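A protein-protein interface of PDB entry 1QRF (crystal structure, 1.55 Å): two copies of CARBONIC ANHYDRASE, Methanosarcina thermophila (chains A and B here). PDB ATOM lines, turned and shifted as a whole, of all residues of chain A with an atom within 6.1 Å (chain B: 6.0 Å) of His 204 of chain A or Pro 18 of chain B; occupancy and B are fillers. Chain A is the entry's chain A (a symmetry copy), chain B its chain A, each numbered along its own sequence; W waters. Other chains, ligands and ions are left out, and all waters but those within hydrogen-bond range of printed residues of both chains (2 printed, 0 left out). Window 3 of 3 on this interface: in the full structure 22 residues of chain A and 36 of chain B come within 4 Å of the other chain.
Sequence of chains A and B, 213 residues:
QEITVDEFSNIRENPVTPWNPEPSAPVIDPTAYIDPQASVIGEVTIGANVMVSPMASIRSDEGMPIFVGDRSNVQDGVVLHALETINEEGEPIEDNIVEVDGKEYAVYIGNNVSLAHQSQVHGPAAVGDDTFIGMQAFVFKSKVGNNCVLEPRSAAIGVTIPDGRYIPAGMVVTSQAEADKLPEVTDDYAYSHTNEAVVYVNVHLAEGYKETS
Water W1 bridges the backbone carbonyl oxygen (O) of His 204 of chain A (2.8 Å) and the backbone carbonyl oxygen (O) of Val 16 of chain B (3.1 Å). Water W2 bridges the backbone NH of Val 16 of chain B (2.9 Å) and the backbone carbonyl oxygen of Gly 208 of chain A (2.9 Å).
O of Val 201 of chain A touches CH2 of Trp 19 of chain B (3.7 Å). CD2 of His 204 of chain A touches CG of Pro 18 of chain B (3.6 Å). His 204 of chain A touches Trp 19 of chain B. CG2 of Thr 17 of chain B touches CD2 of Leu 205 of chain A, 3.98 Å away. CZ2 of Trp 19 of chain B touches CD2 of Leu 205 of chain A (3.9 Å). Gly 208 of chain A touches Val 16 of chain B (CA to O, 3.5 Å).
No position is printed for both chains. Of the 6 pairs that touch across the chains among the printed residues, none has its exchanged pair printed and touching as well.
Tyr 200 of chain A touches none of the printed residues of chain B. His 204 of chain A touches just these residues of chain B: Pro 18 and Trp 19. Of the printed residues of chain A, Val 16 of chain B touches Gly 208 (3.5 Å). Of the printed residues of chain A, Thr 17 of chain B touches Leu 205. Pro 18 of chain B touches one residue of chain A. The nearest residue of chain A that does not touch Pro 18 of chain B is Tyr 200 of chain A (4.1 Å). The nearest printed residue of chain B that does not touch Leu 205 of chain A is Val 16 of chain B (6.2 Å).
The backbone NH (N) of Asn 20 of chain B sits at hydrogen-bond distance from the side-chain hydroxyl (OG1) of Thr 17 of chain B. The backbone carbonyl oxygen (O) of Tyr 200 of chain A sits at hydrogen-bond distance from a ring nitrogen (ND1) of His 204 of chain A, at 2.8 Å. OG1 of Thr 17 of chain B sits close to NE1 of Trp 19 of chain B (3.3 Å).
Of the 11 printed residues of chain A, 4 touch a printed residue of chain B.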
ATOM      1  N   VAL A 199       8.346   1.754   3.759  1.00  0.00           N
ATOM      2  CA  VAL A 199       8.270   1.908   2.312  1.00  0.00           C
ATOM      3  C   VAL A 199       8.637   0.577   1.645  1.00  0.00           C
ATOM      4  O   VAL A 199       7.903   0.113   0.743  1.00  0.00           O
ATOM      5  CB  VAL A 199       9.251   3.020   1.861  1.00  0.00           C
ATOM      6  CG1 VAL A 199       9.435   2.983   0.353  1.00  0.00           C
ATOM      7  CG2 VAL A 199       8.638   4.356   2.288  1.00  0.00           C
ATOM      8  N   TYR A 200       9.648  -0.115   2.175  1.00  0.00           N
ATOM      9  CA  TYR A 200       9.969  -1.428   1.594  1.00  0.00           C
ATOM     10  C   TYR A 200       8.778  -2.381   1.678  1.00  0.00           C
ATOM     11  O   TYR A 200       8.334  -3.023   0.694  1.00  0.00           O
ATOM     12  CB  TYR A 200      11.169  -2.046   2.318  1.00  0.00           C
ATOM     13  CG  TYR A 200      11.237  -3.557   2.242  1.00  0.00           C
ATOM     14  CD1 TYR A 200      11.901  -4.210   1.243  1.00  0.00           C
ATOM     15  CD2 TYR A 200      10.587  -4.321   3.203  1.00  0.00           C
ATOM     16  CE1 TYR A 200      11.946  -5.595   1.187  1.00  0.00           C
ATOM     17  CE2 TYR A 200      10.592  -5.703   3.174  1.00  0.00           C
ATOM     18  CZ  TYR A 200      11.275  -6.328   2.143  1.00  0.00           C
ATOM     19  OH  TYR A 200      11.295  -7.705   2.076  1.00  0.00           O
ATOM     20  N   VAL A 201       8.198  -2.421   2.866  1.00  0.00           N
ATOM     21  CA  VAL A 201       7.022  -3.314   3.089  1.00  0.00           C
ATOM     22  C   VAL A 201       5.899  -2.942   2.172  1.00  0.00           C
ATOM     23  O   VAL A 201       5.229  -3.728   1.495  1.00  0.00           O
ATOM     24  CB  VAL A 201       6.572  -3.220   4.562  1.00  0.00           C
ATOM     25  CG1 VAL A 201       5.241  -3.960   4.757  1.00  0.00           C
ATOM     26  CG2 VAL A 201       7.664  -3.811   5.430  1.00  0.00           C
ATOM     27  N   ASN A 202       5.533  -1.656   2.123  1.00  0.00           N
ATOM     28  CA  ASN A 202       4.400  -1.175   1.365  1.00  0.00           C
ATOM     29  C   ASN A 202       4.520  -1.257  -0.127  1.00  0.00           C
ATOM     30  O   ASN A 202       3.566  -1.569  -0.829  1.00  0.00           O
ATOM     31  CB  ASN A 202       3.947   0.232   1.807  1.00  0.00           C
ATOM     32  CG  ASN A 202       3.117   0.173   3.089  1.00  0.00           C
ATOM     33  OD1 ASN A 202       1.884   0.141   2.945  1.00  0.00           O
ATOM     34  ND2 ASN A 202       3.777   0.136   4.233  1.00  0.00           N
ATOM     35  N   VAL A 203       5.756  -1.094  -0.668  1.00  0.00           N
ATOM     36  CA  VAL A 203       5.924  -1.361  -2.108  1.00  0.00           C
ATOM     37  C   VAL A 203       5.727  -2.840  -2.405  1.00  0.00           C
ATOM     38  O   VAL A 203       5.064  -3.175  -3.400  1.00  0.00           O
ATOM     39  CB  VAL A 203       7.373  -0.927  -2.436  1.00  0.00           C
ATOM     40  CG1 VAL A 203       7.923  -1.517  -3.710  1.00  0.00           C
ATOM     41  CG2 VAL A 203       7.432   0.586  -2.458  1.00  0.00           C
ATOM     42  N   HIS A 204       6.177  -3.716  -1.519  1.00  0.00           N
ATOM     43  CA  HIS A 204       5.894  -5.151  -1.709  1.00  0.00           C
ATOM     44  C   HIS A 204       4.430  -5.471  -1.511  1.00  0.00           C
ATOM     45  O   HIS A 204       3.882  -6.317  -2.259  1.00  0.00           O
ATOM     46  CB  HIS A 204       6.789  -5.995  -0.791  1.00  0.00           C
ATOM     47  CG  HIS A 204       8.216  -6.069  -1.285  1.00  0.00           C
ATOM     48  ND1 HIS A 204       9.149  -5.087  -0.997  1.00  0.00           N
ATOM     49  CD2 HIS A 204       8.845  -6.982  -2.071  1.00  0.00           C
ATOM     50  CE1 HIS A 204      10.294  -5.425  -1.589  1.00  0.00           C
ATOM     51  NE2 HIS A 204      10.144  -6.583  -2.227  1.00  0.00           N
ATOM     52  N   LEU A 205       3.713  -4.830  -0.597  1.00  0.00           N
ATOM     53  CA  LEU A 205       2.281  -5.084  -0.442  1.00  0.00           C
ATOM     54  C   LEU A 205       1.506  -4.616  -1.655  1.00  0.00           C
ATOM     55  O   LEU A 205       0.582  -5.296  -2.156  1.00  0.00           O
ATOM     56  CB  LEU A 205       1.772  -4.384   0.832  1.00  0.00           C
ATOM     57  CG  LEU A 205       2.050  -5.065   2.141  1.00  0.00           C
ATOM     58  CD1 LEU A 205       1.548  -4.154   3.288  1.00  0.00           C
ATOM     59  CD2 LEU A 205       1.339  -6.424   2.253  1.00  0.00           C
ATOM     60  N   ALA A 206       1.817  -3.448  -2.230  1.00  0.00           N
ATOM     61  CA  ALA A 206       1.132  -2.969  -3.413  1.00  0.00           C
ATOM     62  C   ALA A 206       1.251  -4.035  -4.521  1.00  0.00           C
ATOM     63  O   ALA A 206       0.271  -4.380  -5.195  1.00  0.00           O
ATOM     64  CB  ALA A 206       1.698  -1.641  -3.915  1.00  0.00           C
ATOM     65  N   GLU A 207       2.449  -4.566  -4.736  1.00  0.00           N
ATOM     66  CA  GLU A 207       2.625  -5.580  -5.792  1.00  0.00           C
ATOM     67  C   GLU A 207       1.880  -6.868  -5.440  1.00  0.00           C
ATOM     68  O   GLU A 207       1.222  -7.438  -6.331  1.00  0.00           O
ATOM     69  CB  GLU A 207       4.110  -5.866  -5.995  1.00  0.00           C
ATOM     70  CG  GLU A 207       4.387  -7.060  -6.939  1.00  0.00           C
ATOM     71  CD  GLU A 207       3.904  -6.778  -8.333  1.00  0.00           C
ATOM     72  OE1 GLU A 207       3.626  -5.620  -8.695  1.00  0.00           O
ATOM     73  OE2 GLU A 207       3.738  -7.722  -9.159  1.00  0.00           O
ATOM     74  N   GLY A 208       1.925  -7.345  -4.205  1.00  0.00           N
ATOM     75  CA  GLY A 208       1.167  -8.549  -3.854  1.00  0.00           C
ATOM     76  C   GLY A 208      -0.316  -8.319  -4.042  1.00  0.00           C
ATOM     77  O   GLY A 208      -1.075  -9.132  -4.605  1.00  0.00           O
ATOM     78  N   TYR A 209      -0.829  -7.148  -3.588  1.00  0.00           N
ATOM     79  CA  TYR A 209      -2.254  -6.879  -3.763  1.00  0.00           C
ATOM     80  C   TYR A 209      -2.615  -6.735  -5.241  1.00  0.00           C
ATOM     81  O   TYR A 209      -3.670  -7.134  -5.698  1.00  0.00           O
ATOM     82  CB  TYR A 209      -2.703  -5.613  -3.005  1.00  0.00           C
ATOM     83  CG  TYR A 209      -2.965  -5.886  -1.536  1.00  0.00           C
ATOM     84  CD1 TYR A 209      -2.169  -5.274  -0.559  1.00  0.00           C
ATOM     85  CD2 TYR A 209      -4.010  -6.667  -1.112  1.00  0.00           C
ATOM     86  CE1 TYR A 209      -2.370  -5.483   0.801  1.00  0.00           C
ATOM     87  CE2 TYR A 209      -4.224  -6.916   0.222  1.00  0.00           C
ATOM     88  CZ  TYR A 209      -3.437  -6.277   1.185  1.00  0.00           C
ATOM     89  OH  TYR A 209      -3.683  -6.535   2.515  1.00  0.00           O
ATOM     90  N   VAL B  16       0.393 -12.551  -1.423  1.00  0.00           N
ATOM     91  CA  VAL B  16       1.695 -13.228  -1.340  1.00  0.00           C
ATOM     92  C   VAL B  16       2.788 -12.155  -1.316  1.00  0.00           C
ATOM     93  O   VAL B  16       2.709 -11.141  -2.046  1.00  0.00           O
ATOM     94  CB  VAL B  16       1.919 -14.189  -2.524  1.00  0.00           C
ATOM     95  CG1 VAL B  16       3.278 -14.876  -2.457  1.00  0.00           C
ATOM     96  CG2 VAL B  16       0.837 -15.271  -2.588  1.00  0.00           C
ATOM     97  N   THR B  17       3.740 -12.264  -0.412  1.00  0.00           N
ATOM     98  CA  THR B  17       4.831 -11.291  -0.307  1.00  0.00           C
ATOM     99  C   THR B  17       6.058 -12.115   0.035  1.00  0.00           C
ATOM    100  O   THR B  17       5.911 -13.297   0.348  1.00  0.00           O
ATOM    101  CB  THR B  17       4.581 -10.335   0.884  1.00  0.00           C
ATOM    102  OG1 THR B  17       4.552 -11.073   2.104  1.00  0.00           O
ATOM    103  CG2 THR B  17       3.293  -9.542   0.739  1.00  0.00           C
ATOM    104  N   PRO B  18       7.205 -11.505   0.196  1.00  0.00           N
ATOM    105  CA  PRO B  18       8.409 -12.193   0.636  1.00  0.00           C
ATOM    106  C   PRO B  18       8.322 -12.788   2.015  1.00  0.00           C
ATOM    107  O   PRO B  18       9.079 -13.718   2.337  1.00  0.00           O
ATOM    108  CB  PRO B  18       9.559 -11.167   0.619  1.00  0.00           C
ATOM    109  CG  PRO B  18       8.994 -10.122  -0.311  1.00  0.00           C
ATOM    110  CD  PRO B  18       7.489 -10.107  -0.157  1.00  0.00           C
ATOM    111  N   TRP B  19       7.463 -12.330   2.908  1.00  0.00           N
ATOM    112  CA  TRP B  19       7.281 -12.832   4.249  1.00  0.00           C
ATOM    113  C   TRP B  19       5.973 -13.612   4.378  1.00  0.00           C
ATOM    114  O   TRP B  19       5.611 -14.074   5.459  1.00  0.00           O
ATOM    115  CB  TRP B  19       7.265 -11.669   5.272  1.00  0.00           C
ATOM    116  CG  TRP B  19       6.165 -10.677   5.016  1.00  0.00           C
ATOM    117  CD1 TRP B  19       4.874 -10.709   5.476  1.00  0.00           C
ATOM    118  CD2 TRP B  19       6.289  -9.482   4.242  1.00  0.00           C
ATOM    119  NE1 TRP B  19       4.193  -9.614   4.988  1.00  0.00           N
ATOM    120  CE2 TRP B  19       5.023  -8.849   4.218  1.00  0.00           C
ATOM    121  CE3 TRP B  19       7.351  -8.896   3.531  1.00  0.00           C
ATOM    122  CZ2 TRP B  19       4.799  -7.658   3.540  1.00  0.00           C
ATOM    123  CZ3 TRP B  19       7.115  -7.724   2.843  1.00  0.00           C
ATOM    124  CH2 TRP B  19       5.856  -7.103   2.865  1.00  0.00           C
ATOM    125  N   ASN B  20       5.275 -13.809   3.261  1.00  0.00           N
ATOM    126  CA  ASN B  20       3.998 -14.530   3.299  1.00  0.00           C
ATOM    127  C   ASN B  20       3.827 -15.440   2.104  1.00  0.00           C
ATOM    128  O   ASN B  20       3.154 -15.116   1.123  1.00  0.00           O
ATOM    129  CB  ASN B  20       2.828 -13.527   3.321  1.00  0.00           C
ATOM    130  CG  ASN B  20       1.510 -14.204   3.651  1.00  0.00           C
ATOM    131  OD1 ASN B  20       1.435 -14.976   4.598  1.00  0.00           O
ATOM    132  ND2 ASN B  20       0.451 -13.986   2.889  1.00  0.00           N
ATOM    133  N   PRO B  21       4.501 -16.586   2.124  1.00  0.00           N
ATOM    134  CA  PRO B  21       4.505 -17.559   1.050  1.00  0.00           C
ATOM    135  C   PRO B  21       3.157 -18.207   0.797  1.00  0.00           C
ATOM    136  O   PRO B  21       2.734 -18.414  -0.344  1.00  0.00           O
ATOM    137  CB  PRO B  21       5.496 -18.683   1.453  1.00  0.00           C
ATOM    138  CG  PRO B  21       5.664 -18.457   2.931  1.00  0.00           C
ATOM    139  CD  PRO B  21       5.341 -17.013   3.251  1.00  0.00           C
ATOM    140  N   ILE B  86       8.193 -11.183  10.369  1.00  0.00           N
ATOM    141  CA  ILE B  86       9.137 -12.054   9.654  1.00  0.00           C
ATOM    142  C   ILE B  86      10.188 -11.257   8.897  1.00  0.00           C
ATOM    143  O   ILE B  86       9.786 -10.428   8.074  1.00  0.00           O
ATOM    144  CB  ILE B  86       8.343 -12.988   8.729  1.00  0.00           C
ATOM    145  CG1 ILE B  86       7.581 -14.046   9.508  1.00  0.00           C
ATOM    146  CG2 ILE B  86       9.182 -13.659   7.665  1.00  0.00           C
ATOM    147  CD1 ILE B  86       6.175 -14.301   9.063  1.00  0.00           C
HETATM  148  O   HOH W   1       4.788  -8.938  -2.830  1.00  0.00           O
HETATM  149  O   HOH W   2      -0.833 -11.999  -3.958  1.00  0.00           O
